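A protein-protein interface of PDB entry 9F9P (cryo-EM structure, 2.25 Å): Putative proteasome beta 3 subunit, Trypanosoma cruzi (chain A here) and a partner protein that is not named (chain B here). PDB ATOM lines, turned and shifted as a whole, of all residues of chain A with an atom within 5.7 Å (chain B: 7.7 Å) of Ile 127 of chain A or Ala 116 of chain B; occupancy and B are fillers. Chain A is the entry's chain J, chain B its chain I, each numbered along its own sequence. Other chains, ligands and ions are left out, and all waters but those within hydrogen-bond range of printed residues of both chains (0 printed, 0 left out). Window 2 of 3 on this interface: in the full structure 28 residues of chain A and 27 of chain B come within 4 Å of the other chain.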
ATOM      1  N   SER A  92       7.907  17.341  -5.939  1.00  0.00           N
ATOM      2  CA  SER A  92       8.231  18.646  -5.366  1.00  0.00           C
ATOM      3  C   SER A  92       9.139  18.538  -4.155  1.00  0.00           C
ATOM      4  O   SER A  92      10.059  19.315  -3.992  1.00  0.00           O
ATOM      5  CB  SER A  92       6.927  19.318  -5.058  1.00  0.00           C
ATOM      6  OG  SER A  92       7.043  20.451  -4.197  1.00  0.00           O
ATOM      7  N   LEU A  95      12.782  17.757  -5.424  1.00  0.00           N
ATOM      8  CA  LEU A  95      13.441  18.962  -5.932  1.00  0.00           C
ATOM      9  C   LEU A  95      13.866  19.933  -4.833  1.00  0.00           C
ATOM     10  O   LEU A  95      14.918  20.533  -4.981  1.00  0.00           O
ATOM     11  CB  LEU A  95      12.538  19.697  -6.923  1.00  0.00           C
ATOM     12  CG  LEU A  95      12.209  18.909  -8.202  1.00  0.00           C
ATOM     13  CD1 LEU A  95      11.205  19.592  -9.080  1.00  0.00           C
ATOM     14  CD2 LEU A  95      13.471  18.677  -9.003  1.00  0.00           C
ATOM     15  N   TYR A  96      13.037  20.141  -3.786  1.00  0.00           N
ATOM     16  CA  TYR A  96      13.342  21.106  -2.729  1.00  0.00           C
ATOM     17  C   TYR A  96      14.484  20.573  -1.861  1.00  0.00           C
ATOM     18  O   TYR A  96      15.347  21.340  -1.478  1.00  0.00           O
ATOM     19  CB  TYR A  96      12.113  21.473  -1.869  1.00  0.00           C
ATOM     20  CG  TYR A  96      12.276  22.713  -1.024  1.00  0.00           C
ATOM     21  CD1 TYR A  96      12.174  23.985  -1.593  1.00  0.00           C
ATOM     22  CD2 TYR A  96      12.608  22.639   0.331  1.00  0.00           C
ATOM     23  CE1 TYR A  96      12.373  25.146  -0.842  1.00  0.00           C
ATOM     24  CE2 TYR A  96      12.825  23.792   1.100  1.00  0.00           C
ATOM     25  CZ  TYR A  96      12.725  25.050   0.507  1.00  0.00           C
ATOM     26  OH  TYR A  96      12.914  26.210   1.244  1.00  0.00           O
ATOM     27  N   ALA A  98      17.121  19.601  -2.945  1.00  0.00           N
ATOM     28  CA  ALA A  98      18.334  20.153  -3.545  1.00  0.00           C
ATOM     29  C   ALA A  98      18.244  21.671  -3.737  1.00  0.00           C
ATOM     30  O   ALA A  98      18.682  22.218  -4.730  1.00  0.00           O
ATOM     31  CB  ALA A  98      18.534  19.428  -4.859  1.00  0.00           C
ATOM     32  N   ARG A  99      17.632  22.363  -2.776  1.00  0.00           N
ATOM     33  CA  ARG A  99      17.277  23.769  -2.879  1.00  0.00           C
ATOM     34  C   ARG A  99      18.482  24.611  -3.254  1.00  0.00           C
ATOM     35  O   ARG A  99      18.350  25.520  -4.069  1.00  0.00           O
ATOM     36  CB  ARG A  99      16.731  24.276  -1.529  1.00  0.00           C
ATOM     37  CG  ARG A  99      16.566  25.795  -1.402  1.00  0.00           C
ATOM     38  CD  ARG A  99      15.505  26.295  -2.358  1.00  0.00           C
ATOM     39  NE  ARG A  99      15.227  27.717  -2.258  1.00  0.00           N
ATOM     40  CZ  ARG A  99      15.966  28.664  -2.816  1.00  0.00           C
ATOM     41  NH1 ARG A  99      15.592  29.918  -2.712  1.00  0.00           N
ATOM     42  NH2 ARG A  99      17.076  28.349  -3.461  1.00  0.00           N
ATOM     43  N   PRO A 102      20.594  22.788  -7.330  1.00  0.00           N
ATOM     44  CA  PRO A 102      19.374  22.169  -7.872  1.00  0.00           C
ATOM     45  C   PRO A 102      19.606  21.183  -9.003  1.00  0.00           C
ATOM     46  O   PRO A 102      20.705  21.135  -9.559  1.00  0.00           O
ATOM     47  CB  PRO A 102      18.487  23.354  -8.277  1.00  0.00           C
ATOM     48  CG  PRO A 102      19.477  24.506  -8.495  1.00  0.00           C
ATOM     49  CD  PRO A 102      20.700  24.220  -7.632  1.00  0.00           C
ATOM     50  N   ASP A 125       8.657  24.561 -11.217  1.00  0.00           N
ATOM     51  CA  ASP A 125       9.994  25.083 -11.450  1.00  0.00           C
ATOM     52  C   ASP A 125      11.058  24.132 -10.889  1.00  0.00           C
ATOM     53  O   ASP A 125      10.770  23.097 -10.315  1.00  0.00           O
ATOM     54  CB  ASP A 125      10.140  26.492 -10.871  1.00  0.00           C
ATOM     55  CG  ASP A 125       9.984  26.581  -9.355  1.00  0.00           C
ATOM     56  OD1 ASP A 125      10.698  25.840  -8.639  1.00  0.00           O
ATOM     57  OD2 ASP A 125       9.178  27.422  -8.892  1.00  0.00           O
ATOM     58  N   LEU A 126      12.321  24.515 -11.023  1.00  0.00           N
ATOM     59  CA  LEU A 126      13.402  23.580 -10.794  1.00  0.00           C
ATOM     60  C   LEU A 126      13.691  23.357  -9.303  1.00  0.00           C
ATOM     61  O   LEU A 126      14.482  22.482  -8.967  1.00  0.00           O
ATOM     62  CB  LEU A 126      14.634  24.055 -11.569  1.00  0.00           C
ATOM     63  CG  LEU A 126      15.602  24.999 -10.856  1.00  0.00           C
ATOM     64  CD1 LEU A 126      16.819  25.245 -11.721  1.00  0.00           C
ATOM     65  CD2 LEU A 126      14.942  26.326 -10.539  1.00  0.00           C
ATOM     66  N   ILE A 127      13.065  24.125  -8.409  1.00  0.00           N
ATOM     67  CA  ILE A 127      13.163  23.848  -6.976  1.00  0.00           C
ATOM     68  C   ILE A 127      11.825  23.422  -6.389  1.00  0.00           C
ATOM     69  O   ILE A 127      11.719  23.285  -5.193  1.00  0.00           O
ATOM     70  CB  ILE A 127      13.720  25.047  -6.196  1.00  0.00           C
ATOM     71  CG1 ILE A 127      12.982  26.341  -6.506  1.00  0.00           C
ATOM     72  CG2 ILE A 127      15.217  25.206  -6.417  1.00  0.00           C
ATOM     73  CD1 ILE A 127      13.359  27.458  -5.531  1.00  0.00           C
ATOM     74  N   GLY A 128      10.811  23.195  -7.212  1.00  0.00           N
ATOM     75  CA  GLY A 128       9.672  22.401  -6.799  1.00  0.00           C
ATOM     76  C   GLY A 128       8.367  23.170  -6.599  1.00  0.00           C
ATOM     77  O   GLY A 128       7.378  22.564  -6.199  1.00  0.00           O
ATOM     78  N   ALA A 129       8.315  24.461  -6.898  1.00  0.00           N
ATOM     79  CA  ALA A 129       7.079  25.208  -6.716  1.00  0.00           C
ATOM     80  C   ALA A 129       6.048  24.806  -7.764  1.00  0.00           C
ATOM     81  O   ALA A 129       6.312  24.920  -8.948  1.00  0.00           O
ATOM     82  CB  ALA A 129       7.343  26.688  -6.799  1.00  0.00           C
ATOM     83  N   GLY B 113       7.217  36.548  -2.300  1.00  0.00           N
ATOM     84  CA  GLY B 113       8.584  36.011  -2.324  1.00  0.00           C
ATOM     85  C   GLY B 113       8.748  34.887  -3.364  1.00  0.00           C
ATOM     86  O   GLY B 113       7.944  34.728  -4.268  1.00  0.00           O
ATOM     87  N   THR B 114       9.783  34.068  -3.193  1.00  0.00           N
ATOM     88  CA  THR B 114       9.987  32.850  -3.956  1.00  0.00           C
ATOM     89  C   THR B 114       8.913  31.822  -3.580  1.00  0.00           C
ATOM     90  O   THR B 114       8.847  31.399  -2.434  1.00  0.00           O
ATOM     91  CB  THR B 114      11.406  32.347  -3.663  1.00  0.00           C
ATOM     92  OG1 THR B 114      12.369  33.338  -4.014  1.00  0.00           O
ATOM     93  CG2 THR B 114      11.728  31.041  -4.361  1.00  0.00           C
ATOM     94  N   ALA B 115       8.079  31.389  -4.537  1.00  0.00           N
ATOM     95  CA  ALA B 115       6.958  30.507  -4.232  1.00  0.00           C
ATOM     96  C   ALA B 115       7.351  29.238  -3.468  1.00  0.00           C
ATOM     97  O   ALA B 115       6.622  28.826  -2.588  1.00  0.00           O
ATOM     98  CB  ALA B 115       6.277  30.124  -5.505  1.00  0.00           C
ATOM     99  N   ALA B 116       8.441  28.569  -3.840  1.00  0.00           N
ATOM    100  CA  ALA B 116       8.814  27.280  -3.272  1.00  0.00           C
ATOM    101  C   ALA B 116       9.169  27.436  -1.794  1.00  0.00           C
ATOM    102  O   ALA B 116       8.963  26.496  -1.037  1.00  0.00           O
ATOM    103  CB  ALA B 116      10.009  26.667  -4.004  1.00  0.00           C
ATOM    104  N   ASP B 117       9.825  28.569  -1.472  1.00  0.00           N
ATOM    105  CA  ASP B 117      10.344  28.882  -0.138  1.00  0.00           C
ATOM    106  C   ASP B 117       9.168  29.167   0.797  1.00  0.00           C
ATOM    107  O   ASP B 117       9.027  28.560   1.847  1.00  0.00           O
ATOM    108  CB  ASP B 117      11.320  30.055  -0.214  1.00  0.00           C
ATOM    109  CG  ASP B 117      12.744  29.675  -0.625  1.00  0.00           C
ATOM    110  OD1 ASP B 117      13.093  28.482  -0.550  1.00  0.00           O
ATOM    111  OD2 ASP B 117      13.511  30.564  -1.060  1.00  0.00           O
ATOM    112  N   THR B 118       8.281  30.036   0.351  1.00  0.00           N
ATOM    113  CA  THR B 118       7.043  30.330   1.036  1.00  0.00           C
ATOM    114  C   THR B 118       6.232  29.075   1.314  1.00  0.00           C
ATOM    115  O   THR B 118       5.725  28.888   2.411  1.00  0.00           O
ATOM    116  CB  THR B 118       6.292  31.376   0.213  1.00  0.00           C
ATOM    117  OG1 THR B 118       6.806  32.663   0.583  1.00  0.00           O
ATOM    118  CG2 THR B 118       4.815  31.349   0.454  1.00  0.00           C
ATOM    119  N   GLU B 119       6.075  28.217   0.308  1.00  0.00           N
ATOM    120  CA  GLU B 119       5.313  26.977   0.453  1.00  0.00           C
ATOM    121  C   GLU B 119       5.955  26.055   1.487  1.00  0.00           C
ATOM    122  O   GLU B 119       5.279  25.528   2.345  1.00  0.00           O
ATOM    123  CB  GLU B 119       5.284  26.246  -0.887  1.00  0.00           C
ATOM    124  CG  GLU B 119       4.158  25.254  -1.002  1.00  0.00           C
ATOM    125  CD  GLU B 119       2.855  25.866  -1.495  1.00  0.00           C
ATOM    126  OE1 GLU B 119       2.589  27.033  -1.155  1.00  0.00           O
ATOM    127  OE2 GLU B 119       2.106  25.158  -2.216  1.00  0.00           O
ATOM    128  N   ALA B 120       7.272  25.882   1.429  1.00  0.00           N
ATOM    129  CA  ALA B 120       7.977  24.948   2.284  1.00  0.00           C
ATOM    130  C   ALA B 120       7.915  25.328   3.757  1.00  0.00           C
ATOM    131  O   ALA B 120       7.639  24.474   4.594  1.00  0.00           O
ATOM    132  CB  ALA B 120       9.401  24.835   1.850  1.00  0.00           C
ATOM    133  N   VAL B 121       8.243  26.582   4.062  1.00  0.00           N
ATOM    134  CA  VAL B 121       8.200  27.151   5.399  1.00  0.00           C
ATOM    135  C   VAL B 121       6.815  27.051   6.034  1.00  0.00           C
ATOM    136  O   VAL B 121       6.702  26.642   7.172  1.00  0.00           O
ATOM    137  CB  VAL B 121       8.657  28.610   5.328  1.00  0.00           C
ATOM    138  CG1 VAL B 121       8.398  29.378   6.582  1.00  0.00           C
ATOM    139  CG2 VAL B 121      10.136  28.656   5.018  1.00  0.00           C
ATOM    140  N   THR B 122       5.772  27.445   5.336  1.00  0.00           N
ATOM    141  CA  THR B 122       4.452  27.393   5.936  1.00  0.00           C
ATOM    142  C   THR B 122       3.982  25.953   6.168  1.00  0.00           C
ATOM    143  O   THR B 122       3.302  25.724   7.154  1.00  0.00           O
ATOM    144  CB  THR B 122       3.417  28.167   5.113  1.00  0.00           C
ATOM    145  OG1 THR B 122       3.364  27.710   3.772  1.00  0.00           O
ATOM    146  CG2 THR B 122       3.776  29.636   5.083  1.00  0.00           C
ATOM    147  N   ASN B 123       4.320  25.009   5.291  1.00  0.00           N
ATOM    148  CA  ASN B 123       3.991  23.611   5.523  1.00  0.00           C
ATOM    149  C   ASN B 123       4.705  23.021   6.738  1.00  0.00           C
ATOM    150  O   ASN B 123       4.113  22.260   7.478  1.00  0.00           O
ATOM    151  CB  ASN B 123       4.257  22.729   4.304  1.00  0.00           C
ATOM    152  CG  ASN B 123       3.219  23.009   3.239  1.00  0.00           C
ATOM    153  OD1 ASN B 123       2.069  23.325   3.530  1.00  0.00           O
ATOM    154  ND2 ASN B 123       3.645  23.002   1.994  1.00  0.00           N
ATOM    155  N   VAL B 160      16.386  31.762   2.288  1.00  0.00           N
ATOM    156  CA  VAL B 160      15.020  31.306   2.121  1.00  0.00           C
ATOM    157  C   VAL B 160      14.125  32.546   2.053  1.00  0.00           C
ATOM    158  O   VAL B 160      13.810  33.126   3.081  1.00  0.00           O
ATOM    159  CB  VAL B 160      14.609  30.319   3.244  1.00  0.00           C
ATOM    160  CG1 VAL B 160      13.103  30.019   3.251  1.00  0.00           C
ATOM    161  CG2 VAL B 160      15.396  29.006   3.184  1.00  0.00           C
ATOM    162  N   SER B 161      13.776  32.988   0.840  1.00  0.00           N
ATOM    163  CA  SER B 161      13.215  34.315   0.651  1.00  0.00           C
ATOM    164  C   SER B 161      11.687  34.261   0.628  1.00  0.00           C
ATOM    165  O   SER B 161      11.055  34.209  -0.408  1.00  0.00           O
ATOM    166  CB  SER B 161      13.792  35.033  -0.548  1.00  0.00           C
ATOM    167  OG  SER B 161      14.149  34.119  -1.561  1.00  0.00           O
ATOM    168  N   ALA B 162      11.122  34.290   1.833  1.00  0.00           N
ATOM    169  CA  ALA B 162       9.693  34.294   2.058  1.00  0.00           C
ATOM    170  C   ALA B 162       9.307  35.531   2.859  1.00  0.00           C
ATOM    171  O   ALA B 162       9.825  35.727   3.936  1.00  0.00           O
ATOM    172  CB  ALA B 162       9.365  33.013   2.793  1.00  0.00           C
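The side-chain hydroxyl of Tyr 96 of chain A is in hydrogen-bond range of the side-chain carboxylate of Asp 117 of chain B (2.9 Å).
The guanidinium group (NH1) of Arg 99 of chain A is in salt-bridge range of the side-chain carboxylate (OD2) of Asp 117 of chain B (2.7 Å).
The backbone NH (N) of Ala 129 of chain A lies within hydrogen-bond range of the side-chain carboxylate (OD1) of Asp 125 of chain A, at 3.3 Å.
The side-chain carboxylate (OD2) of Asp 117 of chain B sits at hydrogen-bond distance from the backbone NH (N) of Ser 161 of chain B (3.1 Å).
The backbone NH of Ile 127 of chain A sits at hydrogen-bond distance from the side-chain carboxylate of Asp 125 of chain A, at 2.9 Å.
Among the printed residues, merely in contact across the chains: Tyr 96 of chain A with Ala 120 of chain B (3.6 Å), Tyr 96 of chain A with Ala 116 of chain B (3.7 Å), Ala 129 of chain A with Ala 116 of chain B (3.7 Å), Ile 127 of chain A with Ala 116 of chain B (3.8 Å) and Ala 129 of chain A with Ala 115 of chain B (3.8 Å).
Of the printed residues of chain B, Ile 127 of chain A touches Ala 116.
Of chain A, only Tyr 96, Ile 127 and Ala 129 come within 4 Å of Ala 116 of chain B.
Of the printed residues of chain A, Asp 117 of chain B touches Tyr 96 (2.9 Å) and Arg 99 (2.7 Å).
Of the printed residues of chain B, Arg 99 of chain A touches Asp 117.
Val 121 of chain B touches none of the printed residues of chain A.
Asp 125 of chain A touches none of the printed residues of chain B.
The nearest residue of chain B that does not touch Ile 127 of chain A is Thr 114 of chain B (4.1 Å).
Of the 11 printed residues of chain A, 4 touch a printed residue of chain B.
Hydrophobic or aromatic side chains of chain A that line the printed part of chain B: Tyr 96, Ile 127 and Ala 129.
Among the printed residues, Asp or Glu carboxylates within 4 Å of a Lys or Arg side-chain nitrogen of the other chain: Arg 99 of chain A with Asp 117 of chain B (2.7 Å).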
